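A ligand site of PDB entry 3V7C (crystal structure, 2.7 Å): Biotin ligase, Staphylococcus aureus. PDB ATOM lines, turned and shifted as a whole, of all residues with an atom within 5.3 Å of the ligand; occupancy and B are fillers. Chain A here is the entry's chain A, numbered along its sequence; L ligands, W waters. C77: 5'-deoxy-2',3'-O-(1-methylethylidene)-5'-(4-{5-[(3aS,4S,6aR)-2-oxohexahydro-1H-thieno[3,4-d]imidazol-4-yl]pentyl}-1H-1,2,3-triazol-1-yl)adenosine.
The backbone NH of Arg 120 is in hydrogen-bond range of an oxygen (OAD) of the ligand, at 3.0 Å.
N of Ser 128 lies within hydrogen-bond range of N7 of the ligand (3.2 Å).
The side-chain hydroxyl (OG) of Ser 93 is in hydrogen-bond range of an oxygen (OAD) of the ligand (2.9 Å).
The backbone NH (N) of Gly 210 lies close to a sulfur (SAY) of the ligand (3.8 Å).
The side-chain amide oxygen (OE1) of Gln 116 is in hydrogen-bond range of a nitrogen (NAT) of the ligand (2.8 Å).
A nitrogen (NAT) of the ligand sits at hydrogen-bond distance from the side-chain hydroxyl (OG1) of Thr 94 (3.1 Å).
A nitrogen (N6) of the ligand lies within hydrogen-bond range of the backbone carbonyl oxygen (O) of Ser 128.
OD1 of Asn 212 sits close to N1 of the ligand.
The backbone carbonyl oxygen of Arg 120 is in hydrogen-bond range of a nitrogen (NAU) of the ligand (2.7 Å).
ND2 of Asn 212 lies close to NE2 of Gln 215.
The backbone NH (N) of Lys 187 lies within hydrogen-bond range of the backbone carbonyl oxygen (O) of Arg 227.
The side-chain amide nitrogen (NE2) of Gln 95 lies within hydrogen-bond range of the side-chain hydroxyl (OG) of Ser 138 (2.5 Å).
The backbone carbonyl oxygen of Gly 210 lies within hydrogen-bond range of the backbone NH of Gly 190 (2.9 Å).
N of Ile 209 lies within hydrogen-bond range of O of Met 137, at 2.9 Å.
The backbone NH of Thr 229 is in hydrogen-bond range of the backbone carbonyl oxygen of Lys 187.
The backbone carbonyl oxygen (O) of Phe 191 sits close to the side-chain amide oxygen (OD1) of Asn 179 (3.1 Å).
The backbone NH (N) of Trp 127 sits at hydrogen-bond distance from the backbone carbonyl oxygen (O) of Gly 119 (2.8 Å).
The guanidinium group (NH1) of Arg 125 lies close to a nitrogen (NBJ) of the ligand (3.5 Å).
Gln 95 touches the ligand.
Gly 119 touches the ligand (CA to OAD, 3.5 Å).
Gly 121 touches the ligand.
Arg 122 touches the ligand.
His 126 touches the ligand.
Trp 127 touches the ligand.
C of Trp 136 touches CAM of the ligand, 3.98 Å away.
O of Met 137 touches CAM of the ligand, 3.3 Å away.
OG of Ser 138 touches CBM of the ligand, at 3.8 Å.
Lys 187 touches the ligand (O to C2, 3.6 Å).
Gly 190 touches the ligand (O to CAJ, 3.3 Å).
N of Phe 191 touches CAI of the ligand (3.4 Å).
Gly 208 touches the ligand (C to CBN, 3.7 Å).
Ile 209 touches the ligand (O to CAM, 3.6 Å).
Ile 224 touches the ligand.
NH2 of Arg 227 touches CAB of the ligand, at 3.0 Å.
CB of Ala 228 touches C2 of the ligand, 3.8 Å away.
Hydrophobic or aromatic side chains that line the ligand: Trp 127, Ile 224 and Ala 228.
Water W2 lies within hydrogen-bond range of N3 of the ligand and O of Arg 227.
Water W1 lies within hydrogen-bond range of OG of Ser 93 (3.0 Å) and OAD of the ligand (3.5 Å).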
ATOM      1  N   SER A  93      16.000  -2.722  15.575  1.00  0.00           N
ATOM      2  CA  SER A  93      14.889  -2.622  16.486  1.00  0.00           C
ATOM      3  C   SER A  93      13.617  -3.167  15.861  1.00  0.00           C
ATOM      4  O   SER A  93      13.291  -2.830  14.717  1.00  0.00           O
ATOM      5  CB  SER A  93      14.668  -1.146  16.861  1.00  0.00           C
ATOM      6  OG  SER A  93      13.369  -0.978  17.413  1.00  0.00           O
ATOM      7  N   THR A  94      12.860  -3.968  16.585  1.00  0.00           N
ATOM      8  CA  THR A  94      11.582  -4.450  16.032  1.00  0.00           C
ATOM      9  C   THR A  94      10.619  -3.283  15.732  1.00  0.00           C
ATOM     10  O   THR A  94       9.749  -3.379  14.884  1.00  0.00           O
ATOM     11  CB  THR A  94      10.867  -5.377  16.999  1.00  0.00           C
ATOM     12  OG1 THR A  94      10.667  -4.671  18.221  1.00  0.00           O
ATOM     13  CG2 THR A  94      11.681  -6.636  17.291  1.00  0.00           C
ATOM     14  N   GLN A  95      10.785  -2.177  16.456  1.00  0.00           N
ATOM     15  CA  GLN A  95       9.938  -0.986  16.301  1.00  0.00           C
ATOM     16  C   GLN A  95      10.225  -0.283  14.987  1.00  0.00           C
ATOM     17  O   GLN A  95       9.303   0.039  14.253  1.00  0.00           O
ATOM     18  CB  GLN A  95      10.090  -0.024  17.488  1.00  0.00           C
ATOM     19  CG  GLN A  95       8.901   0.881  17.729  1.00  0.00           C
ATOM     20  CD  GLN A  95       7.634   0.231  18.357  1.00  0.00           C
ATOM     21  OE1 GLN A  95       6.723   0.922  18.741  1.00  0.00           O
ATOM     22  NE2 GLN A  95       7.578  -1.061  18.436  1.00  0.00           N
ATOM     23  N   GLN A 116      18.202  -7.061  19.742  1.00  0.00           N
ATOM     24  CA  GLN A 116      18.142  -5.774  19.042  1.00  0.00           C
ATOM     25  C   GLN A 116      19.457  -5.080  19.246  1.00  0.00           C
ATOM     26  O   GLN A 116      19.978  -5.004  20.364  1.00  0.00           O
ATOM     27  CB  GLN A 116      16.997  -4.884  19.537  1.00  0.00           C
ATOM     28  CG  GLN A 116      15.612  -5.500  19.379  1.00  0.00           C
ATOM     29  CD  GLN A 116      14.474  -4.672  19.931  1.00  0.00           C
ATOM     30  OE1 GLN A 116      13.518  -4.302  19.206  1.00  0.00           O
ATOM     31  NE2 GLN A 116      14.570  -4.372  21.223  1.00  0.00           N
ATOM     32  N   LYS A 118      19.829  -1.834  18.352  1.00  0.00           N
ATOM     33  CA  LYS A 118      19.512  -0.420  18.599  1.00  0.00           C
ATOM     34  C   LYS A 118      18.120  -0.248  19.234  1.00  0.00           C
ATOM     35  O   LYS A 118      17.269   0.579  18.782  1.00  0.00           O
ATOM     36  CB  LYS A 118      19.589   0.350  17.297  1.00  0.00           C
ATOM     37  CG  LYS A 118      19.408   1.814  17.478  1.00  0.00           C
ATOM     38  CD  LYS A 118      19.878   2.544  16.243  1.00  0.00           C
ATOM     39  CE  LYS A 118      20.024   4.045  16.510  1.00  0.00           C
ATOM     40  NZ  LYS A 118      20.851   4.637  15.422  1.00  0.00           N
ATOM     41  N   GLY A 119      17.867  -1.064  20.249  1.00  0.00           N
ATOM     42  CA  GLY A 119      16.609  -1.024  20.928  1.00  0.00           C
ATOM     43  C   GLY A 119      16.457   0.291  21.652  1.00  0.00           C
ATOM     44  O   GLY A 119      17.325   0.673  22.462  1.00  0.00           O
ATOM     45  N   ARG A 120      15.349   0.970  21.357  1.00  0.00           N
ATOM     46  CA  ARG A 120      14.937   2.222  22.001  1.00  0.00           C
ATOM     47  C   ARG A 120      13.621   2.138  22.724  1.00  0.00           C
ATOM     48  O   ARG A 120      12.686   1.452  22.292  1.00  0.00           O
ATOM     49  CB  ARG A 120      14.849   3.332  20.976  1.00  0.00           C
ATOM     50  CG  ARG A 120      16.198   3.679  20.351  1.00  0.00           C
ATOM     51  CD  ARG A 120      17.238   4.083  21.381  1.00  0.00           C
ATOM     52  NE  ARG A 120      18.497   4.369  20.730  1.00  0.00           N
ATOM     53  CZ  ARG A 120      19.503   3.510  20.743  1.00  0.00           C
ATOM     54  NH1 ARG A 120      19.341   2.341  21.351  1.00  0.00           N
ATOM     55  NH2 ARG A 120      20.641   3.790  20.155  1.00  0.00           N
ATOM     56  N   GLY A 121      13.547   2.855  23.833  1.00  0.00           N
ATOM     57  CA  GLY A 121      12.279   3.069  24.557  1.00  0.00           C
ATOM     58  C   GLY A 121      11.826   4.512  24.318  1.00  0.00           C
ATOM     59  O   GLY A 121      12.028   5.080  23.223  1.00  0.00           O
ATOM     60  N   ARG A 122      11.195   5.093  25.352  1.00  0.00           N
ATOM     61  CA  ARG A 122      10.605   6.440  25.265  1.00  0.00           C
ATOM     62  C   ARG A 122      11.695   7.449  25.280  1.00  0.00           C
ATOM     63  O   ARG A 122      12.773   7.206  25.844  1.00  0.00           O
ATOM     64  CB  ARG A 122       9.700   6.660  26.448  1.00  0.00           C
ATOM     65  CG  ARG A 122       8.515   5.690  26.437  1.00  0.00           C
ATOM     66  CD  ARG A 122       7.609   5.788  27.654  1.00  0.00           C
ATOM     67  NE  ARG A 122       7.127   7.149  27.926  1.00  0.00           N
ATOM     68  CZ  ARG A 122       6.851   7.627  29.157  1.00  0.00           C
ATOM     69  NH1 ARG A 122       7.002   6.836  30.215  1.00  0.00           N
ATOM     70  NH2 ARG A 122       6.420   8.883  29.336  1.00  0.00           N
ATOM     71  N   ARG A 125      15.493   6.613  24.616  1.00  0.00           N
ATOM     72  CA  ARG A 125      16.323   6.070  25.667  1.00  0.00           C
ATOM     73  C   ARG A 125      16.697   4.651  25.300  1.00  0.00           C
ATOM     74  O   ARG A 125      15.936   3.948  24.664  1.00  0.00           O
ATOM     75  CB  ARG A 125      15.508   6.024  26.977  1.00  0.00           C
ATOM     76  CG  ARG A 125      15.525   7.261  27.869  1.00  0.00           C
ATOM     77  CD  ARG A 125      15.689   6.832  29.334  1.00  0.00           C
ATOM     78  NE  ARG A 125      14.820   7.534  30.260  1.00  0.00           N
ATOM     79  CZ  ARG A 125      13.473   7.467  30.250  1.00  0.00           C
ATOM     80  NH1 ARG A 125      12.806   6.735  29.371  1.00  0.00           N
ATOM     81  NH2 ARG A 125      12.766   8.158  31.135  1.00  0.00           N
ATOM     82  N   HIS A 126      17.854   4.209  25.746  1.00  0.00           N
ATOM     83  CA  HIS A 126      18.411   2.922  25.375  1.00  0.00           C
ATOM     84  C   HIS A 126      17.615   1.747  26.004  1.00  0.00           C
ATOM     85  O   HIS A 126      17.311   1.742  27.192  1.00  0.00           O
ATOM     86  CB  HIS A 126      19.909   2.910  25.766  1.00  0.00           C
ATOM     87  CG  HIS A 126      20.479   1.531  25.892  1.00  0.00           C
ATOM     88  ND1 HIS A 126      20.870   0.791  24.794  1.00  0.00           N
ATOM     89  CD2 HIS A 126      20.668   0.740  26.972  1.00  0.00           C
ATOM     90  CE1 HIS A 126      21.284  -0.399  25.182  1.00  0.00           C
ATOM     91  NE2 HIS A 126      21.164  -0.463  26.504  1.00  0.00           N
ATOM     92  N   TRP A 127      17.254   0.752  25.223  1.00  0.00           N
ATOM     93  CA  TRP A 127      16.609  -0.424  25.810  1.00  0.00           C
ATOM     94  C   TRP A 127      17.487  -1.598  25.474  1.00  0.00           C
ATOM     95  O   TRP A 127      17.798  -1.837  24.312  1.00  0.00           O
ATOM     96  CB  TRP A 127      15.205  -0.674  25.252  1.00  0.00           C
ATOM     97  CG  TRP A 127      14.576  -1.883  25.848  1.00  0.00           C
ATOM     98  CD1 TRP A 127      14.574  -3.131  25.340  1.00  0.00           C
ATOM     99  CD2 TRP A 127      13.927  -1.968  27.097  1.00  0.00           C
ATOM    100  NE1 TRP A 127      13.962  -4.008  26.192  1.00  0.00           N
ATOM    101  CE2 TRP A 127      13.552  -3.318  27.278  1.00  0.00           C
ATOM    102  CE3 TRP A 127      13.622  -1.047  28.086  1.00  0.00           C
ATOM    103  CZ2 TRP A 127      12.861  -3.773  28.425  1.00  0.00           C
ATOM    104  CZ3 TRP A 127      12.941  -1.494  29.220  1.00  0.00           C
ATOM    105  CH2 TRP A 127      12.568  -2.856  29.381  1.00  0.00           C
ATOM    106  N   SER A 128      17.875  -2.308  26.508  1.00  0.00           N
ATOM    107  CA  SER A 128      18.803  -3.425  26.471  1.00  0.00           C
ATOM    108  C   SER A 128      18.127  -4.680  25.977  1.00  0.00           C
ATOM    109  O   SER A 128      17.240  -5.197  26.666  1.00  0.00           O
ATOM    110  CB  SER A 128      19.243  -3.691  27.884  1.00  0.00           C
ATOM    111  OG  SER A 128      20.536  -4.193  27.894  1.00  0.00           O
ATOM    112  N   SER A 129      18.542  -5.201  24.822  1.00  0.00           N
ATOM    113  CA  SER A 129      17.849  -6.348  24.240  1.00  0.00           C
ATOM    114  C   SER A 129      18.744  -7.583  24.036  1.00  0.00           C
ATOM    115  O   SER A 129      19.021  -7.955  22.916  1.00  0.00           O
ATOM    116  CB  SER A 129      17.269  -5.898  22.912  1.00  0.00           C
ATOM    117  OG  SER A 129      16.595  -4.695  23.086  1.00  0.00           O
ATOM    118  N   TRP A 136      11.517  -9.490  22.642  1.00  0.00           N
ATOM    119  CA  TRP A 136      11.560  -8.140  22.093  1.00  0.00           C
ATOM    120  C   TRP A 136      10.650  -8.146  20.886  1.00  0.00           C
ATOM    121  O   TRP A 136      10.964  -8.733  19.848  1.00  0.00           O
ATOM    122  CB  TRP A 136      12.983  -7.768  21.670  1.00  0.00           C
ATOM    123  CG  TRP A 136      14.029  -8.310  22.626  1.00  0.00           C
ATOM    124  CD1 TRP A 136      15.103  -9.093  22.300  1.00  0.00           C
ATOM    125  CD2 TRP A 136      14.093  -8.118  24.039  1.00  0.00           C
ATOM    126  NE1 TRP A 136      15.828  -9.383  23.414  1.00  0.00           N
ATOM    127  CE2 TRP A 136      15.235  -8.808  24.492  1.00  0.00           C
ATOM    128  CE3 TRP A 136      13.307  -7.427  24.960  1.00  0.00           C
ATOM    129  CZ2 TRP A 136      15.629  -8.807  25.822  1.00  0.00           C
ATOM    130  CZ3 TRP A 136      13.687  -7.440  26.287  1.00  0.00           C
ATOM    131  CH2 TRP A 136      14.838  -8.117  26.705  1.00  0.00           C
ATOM    132  N   MET A 137       9.518  -7.461  21.005  1.00  0.00           N
ATOM    133  CA  MET A 137       8.479  -7.602  20.023  1.00  0.00           C
ATOM    134  C   MET A 137       7.863  -6.272  19.677  1.00  0.00           C
ATOM    135  O   MET A 137       7.825  -5.360  20.517  1.00  0.00           O
ATOM    136  CB  MET A 137       7.425  -8.518  20.607  1.00  0.00           C
ATOM    137  CG  MET A 137       6.330  -8.754  19.663  1.00  0.00           C
ATOM    138  SD  MET A 137       5.213  -9.971  20.330  1.00  0.00           S
ATOM    139  CE  MET A 137       4.268  -8.992  21.477  1.00  0.00           C
ATOM    140  N   SER A 138       7.373  -6.141  18.454  1.00  0.00           N
ATOM    141  CA  SER A 138       6.519  -5.015  18.167  1.00  0.00           C
ATOM    142  C   SER A 138       5.269  -5.534  17.525  1.00  0.00           C
ATOM    143  O   SER A 138       5.313  -6.382  16.689  1.00  0.00           O
ATOM    144  CB  SER A 138       7.194  -4.054  17.229  1.00  0.00           C
ATOM    145  OG  SER A 138       8.253  -3.429  17.886  1.00  0.00           O
ATOM    146  N   ASN A 179       3.734   2.723  31.417  1.00  0.00           N
ATOM    147  CA  ASN A 179       4.606   2.056  30.449  1.00  0.00           C
ATOM    148  C   ASN A 179       5.528   1.008  30.989  1.00  0.00           C
ATOM    149  O   ASN A 179       6.469   0.599  30.306  1.00  0.00           O
ATOM    150  CB  ASN A 179       5.496   3.128  29.785  1.00  0.00           C
ATOM    151  CG  ASN A 179       4.706   4.035  28.872  1.00  0.00           C
ATOM    152  OD1 ASN A 179       4.133   3.596  27.866  1.00  0.00           O
ATOM    153  ND2 ASN A 179       4.630   5.282  29.221  1.00  0.00           N
ATOM    154  N   ASP A 180       5.347   0.577  32.220  1.00  0.00           N
ATOM    155  CA  ASP A 180       6.277  -0.377  32.756  1.00  0.00           C
ATOM    156  C   ASP A 180       5.595  -1.416  33.619  1.00  0.00           C
ATOM    157  O   ASP A 180       4.494  -1.231  34.094  1.00  0.00           O
ATOM    158  CB  ASP A 180       7.441   0.323  33.442  1.00  0.00           C
ATOM    159  CG  ASP A 180       8.230   1.260  32.475  1.00  0.00           C
ATOM    160  OD1 ASP A 180       7.820   2.405  32.210  1.00  0.00           O
ATOM    161  OD2 ASP A 180       9.284   0.852  31.987  1.00  0.00           O
ATOM    162  N   LYS A 187      11.975  -3.842  37.149  1.00  0.00           N
ATOM    163  CA  LYS A 187      11.312  -3.638  35.872  1.00  0.00           C
ATOM    164  C   LYS A 187      11.513  -4.905  35.029  1.00  0.00           C
ATOM    165  O   LYS A 187      12.650  -5.276  34.708  1.00  0.00           O
ATOM    166  CB  LYS A 187      11.813  -2.385  35.144  1.00  0.00           C
ATOM    167  CG  LYS A 187      10.956  -2.016  33.897  1.00  0.00           C
ATOM    168  CD  LYS A 187      11.571  -0.911  33.044  1.00  0.00           C
ATOM    169  CE  LYS A 187      11.793   0.304  33.932  1.00  0.00           C
ATOM    170  NZ  LYS A 187      11.351   1.576  33.367  1.00  0.00           N
ATOM    171  N   GLY A 190       9.208  -3.180  29.580  1.00  0.00           N
ATOM    172  CA  GLY A 190       8.925  -1.831  29.113  1.00  0.00           C
ATOM    173  C   GLY A 190       8.076  -1.887  27.845  1.00  0.00           C
ATOM    174  O   GLY A 190       8.271  -2.707  26.973  1.00  0.00           O
ATOM    175  N   PHE A 191       7.099  -1.024  27.745  1.00  0.00           N
ATOM    176  CA  PHE A 191       6.372  -0.945  26.489  1.00  0.00           C
ATOM    177  C   PHE A 191       6.054   0.499  26.204  1.00  0.00           C
ATOM    178  O   PHE A 191       6.072   1.362  27.074  1.00  0.00           O
ATOM    179  CB  PHE A 191       5.105  -1.805  26.486  1.00  0.00           C
ATOM    180  CG  PHE A 191       4.118  -1.435  27.562  1.00  0.00           C
ATOM    181  CD1 PHE A 191       4.324  -1.835  28.898  1.00  0.00           C
ATOM    182  CD2 PHE A 191       2.989  -0.672  27.244  1.00  0.00           C
ATOM    183  CE1 PHE A 191       3.432  -1.486  29.892  1.00  0.00           C
ATOM    184  CE2 PHE A 191       2.065  -0.321  28.253  1.00  0.00           C
ATOM    185  CZ  PHE A 191       2.302  -0.735  29.566  1.00  0.00           C
ATOM    186  N   LEU A 192       5.728   0.714  24.963  1.00  0.00           N
ATOM    187  CA  LEU A 192       5.754   1.996  24.338  1.00  0.00           C
ATOM    188  C   LEU A 192       4.725   1.844  23.228  1.00  0.00           C
ATOM    189  O   LEU A 192       4.855   0.946  22.421  1.00  0.00           O
ATOM    190  CB  LEU A 192       7.136   2.103  23.729  1.00  0.00           C
ATOM    191  CG  LEU A 192       7.330   3.103  22.619  1.00  0.00           C
ATOM    192  CD1 LEU A 192       6.915   4.429  23.134  1.00  0.00           C
ATOM    193  CD2 LEU A 192       8.781   3.146  22.246  1.00  0.00           C
ATOM    194  N   GLY A 208       5.535  -1.402  20.763  1.00  0.00           N
ATOM    195  CA  GLY A 208       6.742  -2.177  21.104  1.00  0.00           C
ATOM    196  C   GLY A 208       6.754  -2.570  22.583  1.00  0.00           C
ATOM    197  O   GLY A 208       6.481  -1.745  23.468  1.00  0.00           O
ATOM    198  N   ILE A 209       7.091  -3.837  22.825  1.00  0.00           N
ATOM    199  CA  ILE A 209       6.995  -4.482  24.105  1.00  0.00           C
ATOM    200  C   ILE A 209       8.256  -5.296  24.304  1.00  0.00           C
ATOM    201  O   ILE A 209       8.507  -6.223  23.528  1.00  0.00           O
ATOM    202  CB  ILE A 209       5.841  -5.459  24.114  1.00  0.00           C
ATOM    203  CG1 ILE A 209       4.534  -4.752  23.759  1.00  0.00           C
ATOM    204  CG2 ILE A 209       5.798  -6.294  25.422  1.00  0.00           C
ATOM    205  CD1 ILE A 209       3.408  -5.751  23.536  1.00  0.00           C
ATOM    206  N   GLY A 210       9.033  -4.955  25.333  1.00  0.00           N
ATOM    207  CA  GLY A 210      10.197  -5.717  25.753  1.00  0.00           C
ATOM    208  C   GLY A 210       9.982  -6.291  27.133  1.00  0.00           C
ATOM    209  O   GLY A 210       9.624  -5.583  28.093  1.00  0.00           O
ATOM    210  N   ASN A 212      11.758  -9.031  29.894  1.00  0.00           N
ATOM    211  CA  ASN A 212      12.889  -9.864  30.255  1.00  0.00           C
ATOM    212  C   ASN A 212      12.405 -11.246  30.631  1.00  0.00           C
ATOM    213  O   ASN A 212      11.553 -11.400  31.486  1.00  0.00           O
ATOM    214  CB  ASN A 212      13.658  -9.237  31.404  1.00  0.00           C
ATOM    215  CG  ASN A 212      14.073  -7.794  31.138  1.00  0.00           C
ATOM    216  OD1 ASN A 212      13.785  -6.924  31.957  1.00  0.00           O
ATOM    217  ND2 ASN A 212      14.760  -7.532  30.030  1.00  0.00           N
ATOM    218  N   GLN A 215      17.101 -13.533  32.072  1.00  0.00           N
ATOM    219  CA  GLN A 215      18.364 -12.984  32.587  1.00  0.00           C
ATOM    220  C   GLN A 215      18.532 -13.425  34.016  1.00  0.00           C
ATOM    221  O   GLN A 215      17.537 -13.573  34.721  1.00  0.00           O
ATOM    222  CB  GLN A 215      18.369 -11.454  32.590  1.00  0.00           C
ATOM    223  CG  GLN A 215      18.407 -10.807  31.234  1.00  0.00           C
ATOM    224  CD  GLN A 215      17.018 -10.435  30.742  1.00  0.00           C
ATOM    225  OE1 GLN A 215      16.016 -11.077  31.089  1.00  0.00           O
ATOM    226  NE2 GLN A 215      16.949  -9.361  29.928  1.00  0.00           N
ATOM    227  N   PHE A 220      22.408  -8.399  33.469  1.00  0.00           N
ATOM    228  CA  PHE A 220      21.985  -7.027  33.284  1.00  0.00           C
ATOM    229  C   PHE A 220      23.148  -6.058  33.471  1.00  0.00           C
ATOM    230  O   PHE A 220      23.750  -6.011  34.546  1.00  0.00           O
ATOM    231  CB  PHE A 220      20.925  -6.674  34.317  1.00  0.00           C
ATOM    232  CG  PHE A 220      19.569  -7.252  34.043  1.00  0.00           C
ATOM    233  CD1 PHE A 220      18.857  -6.884  32.911  1.00  0.00           C
ATOM    234  CD2 PHE A 220      18.965  -8.092  34.954  1.00  0.00           C
ATOM    235  CE1 PHE A 220      17.583  -7.379  32.669  1.00  0.00           C
ATOM    236  CE2 PHE A 220      17.684  -8.595  34.711  1.00  0.00           C
ATOM    237  CZ  PHE A 220      16.998  -8.235  33.562  1.00  0.00           C
ATOM    238  N   ILE A 224      21.612  -0.909  35.602  1.00  0.00           N
ATOM    239  CA  ILE A 224      20.176  -1.233  35.728  1.00  0.00           C
ATOM    240  C   ILE A 224      19.878  -2.419  36.655  1.00  0.00           C
ATOM    241  O   ILE A 224      18.717  -2.646  37.045  1.00  0.00           O
ATOM    242  CB  ILE A 224      19.495  -1.370  34.318  1.00  0.00           C
ATOM    243  CG1 ILE A 224      19.735  -2.759  33.710  1.00  0.00           C
ATOM    244  CG2 ILE A 224      19.966  -0.241  33.365  1.00  0.00           C
ATOM    245  CD1 ILE A 224      19.190  -2.946  32.283  1.00  0.00           C
ATOM    246  N   ARG A 227      17.504  -2.209  39.542  1.00  0.00           N
ATOM    247  CA  ARG A 227      16.073  -2.121  39.223  1.00  0.00           C
ATOM    248  C   ARG A 227      15.515  -2.916  38.048  1.00  0.00           C
ATOM    249  O   ARG A 227      14.477  -2.562  37.515  1.00  0.00           O
ATOM    250  CB  ARG A 227      15.475  -0.704  39.315  1.00  0.00           C
ATOM    251  CG  ARG A 227      16.302   0.497  39.024  1.00  0.00           C
ATOM    252  CD  ARG A 227      15.372   1.710  39.357  1.00  0.00           C
ATOM    253  NE  ARG A 227      16.028   3.021  39.294  1.00  0.00           N
ATOM    254  CZ  ARG A 227      16.828   3.435  38.290  1.00  0.00           C
ATOM    255  NH1 ARG A 227      17.387   4.668  38.308  1.00  0.00           N
ATOM    256  NH2 ARG A 227      17.095   2.619  37.260  1.00  0.00           N
ATOM    257  N   ALA A 228      16.162  -4.019  37.683  1.00  0.00           N
ATOM    258  CA  ALA A 228      15.625  -4.845  36.619  1.00  0.00           C
ATOM    259  C   ALA A 228      15.289  -6.245  37.110  1.00  0.00           C
ATOM    260  O   ALA A 228      15.662  -6.622  38.219  1.00  0.00           O
ATOM    261  CB  ALA A 228      16.610  -4.913  35.490  1.00  0.00           C
ATOM    262  N   THR A 229      14.561  -7.002  36.305  1.00  0.00           N
ATOM    263  CA  THR A 229      14.286  -8.377  36.657  1.00  0.00           C
ATOM    264  C   THR A 229      13.777  -9.129  35.463  1.00  0.00           C
ATOM    265  O   THR A 229      13.294  -8.527  34.503  1.00  0.00           O
ATOM    266  CB  THR A 229      13.325  -8.527  37.873  1.00  0.00           C
ATOM    267  OG1 THR A 229      13.402  -9.847  38.387  1.00  0.00           O
ATOM    268  CG2 THR A 229      11.910  -8.221  37.540  1.00  0.00           C
ATOM    269  N   ASP A 322      10.252   8.109  37.987  1.00  0.00           N
ATOM    270  CA  ASP A 322      11.121   7.183  38.750  1.00  0.00           C
ATOM    271  C   ASP A 322      10.553   6.982  40.142  1.00  0.00           C
ATOM    272  O   ASP A 322       9.739   7.764  40.583  1.00  0.00           O
ATOM    273  CB  ASP A 322      12.572   7.686  38.854  1.00  0.00           C
ATOM    274  CG  ASP A 322      13.217   7.950  37.471  1.00  0.00           C
ATOM    275  OD1 ASP A 322      13.089   7.100  36.529  1.00  0.00           O
ATOM    276  OD2 ASP A 322      13.858   9.031  37.336  1.00  0.00           O
HETATM  277  N1  C77 L   1      15.160  -4.265  31.569  1.00  0.00           N
HETATM  278  C2  C77 L   1      14.760  -3.394  32.503  1.00  0.00           C
HETATM  279  N3  C77 L   1      15.013  -2.096  32.405  1.00  0.00           N
HETATM  280  C4  C77 L   1      15.658  -1.625  31.329  1.00  0.00           C
HETATM  281  C5  C77 L   1      16.077  -2.517  30.334  1.00  0.00           C
HETATM  282  C6  C77 L   1      15.811  -3.869  30.479  1.00  0.00           C
HETATM  283  N6  C77 L   1      16.187  -4.767  29.576  1.00  0.00           N
HETATM  284  N7  C77 L   1      16.662  -1.808  29.380  1.00  0.00           N
HETATM  285  C8  C77 L   1      16.623  -0.532  29.758  1.00  0.00           C
HETATM  286  N9  C77 L   1      16.001  -0.398  30.937  1.00  0.00           N
HETATM  287  CAA C77 L   1      17.998   4.019  33.969  1.00  0.00           C
HETATM  288  CAB C77 L   1      15.765   2.998  34.596  1.00  0.00           C
HETATM  289  OAD C77 L   1      13.160  -0.773  20.308  1.00  0.00           O
HETATM  290  CAG C77 L   1      12.277   3.870  27.930  1.00  0.00           C
HETATM  291  CAH C77 L   1      10.643   0.568  25.978  1.00  0.00           C
HETATM  292  CAI C77 L   1       9.669   1.145  27.046  1.00  0.00           C
HETATM  293  CAJ C77 L   1      10.110  -0.663  25.165  1.00  0.00           C
HETATM  294  CAK C77 L   1       9.903   2.689  27.367  1.00  0.00           C
HETATM  295  CAL C77 L   1      11.232  -1.477  24.488  1.00  0.00           C
HETATM  296  CAM C77 L   1      10.761  -4.224  21.569  1.00  0.00           C
HETATM  297  CAN C77 L   1      14.513   3.621  29.323  1.00  0.00           C
HETATM  298  NAR C77 L   1      11.614   2.052  28.824  1.00  0.00           N
HETATM  299  NAS C77 L   1      12.712   2.307  29.265  1.00  0.00           N
HETATM  300  NAT C77 L   1      11.653  -2.446  20.185  1.00  0.00           N
HETATM  301  NAU C77 L   1      11.487  -0.921  21.804  1.00  0.00           N
HETATM  302  OAV C77 L   1      14.661   1.485  30.851  1.00  0.00           O
HETATM  303  OAW C77 L   1      16.143   3.973  32.333  1.00  0.00           O
HETATM  304  OAX C77 L   1      17.296   2.014  32.979  1.00  0.00           O
HETATM  305  SAY C77 L   1      11.782  -3.802  23.007  1.00  0.00           S
HETATM  306  CAZ C77 L   1      12.151  -1.351  20.728  1.00  0.00           C
HETATM  307  CBA C77 L   1      11.272   2.962  27.983  1.00  0.00           C
HETATM  308  CBE C77 L   1      14.839   2.923  30.727  1.00  0.00           C
HETATM  309  CBF C77 L   1      10.634  -2.468  23.481  1.00  0.00           C
HETATM  310  CBG C77 L   1      16.263   3.186  31.131  1.00  0.00           C
HETATM  311  CBH C77 L   1      16.845   1.847  31.613  1.00  0.00           C
HETATM  312  CBI C77 L   1      15.717   0.879  31.656  1.00  0.00           C
HETATM  313  NBJ C77 L   1      13.158   3.327  28.803  1.00  0.00           N
HETATM  314  CBL C77 L   1      16.773   3.254  33.471  1.00  0.00           C
HETATM  315  CBM C77 L   1      10.489  -2.857  20.967  1.00  0.00           C
HETATM  316  CBN C77 L   1      10.387  -1.811  22.092  1.00  0.00           C
HETATM  317  O   HOH W   1      13.046   1.963  18.128  1.00  0.00           O
HETATM  318  O   HOH W   2      14.959  -0.570  34.888  1.00  0.00           O
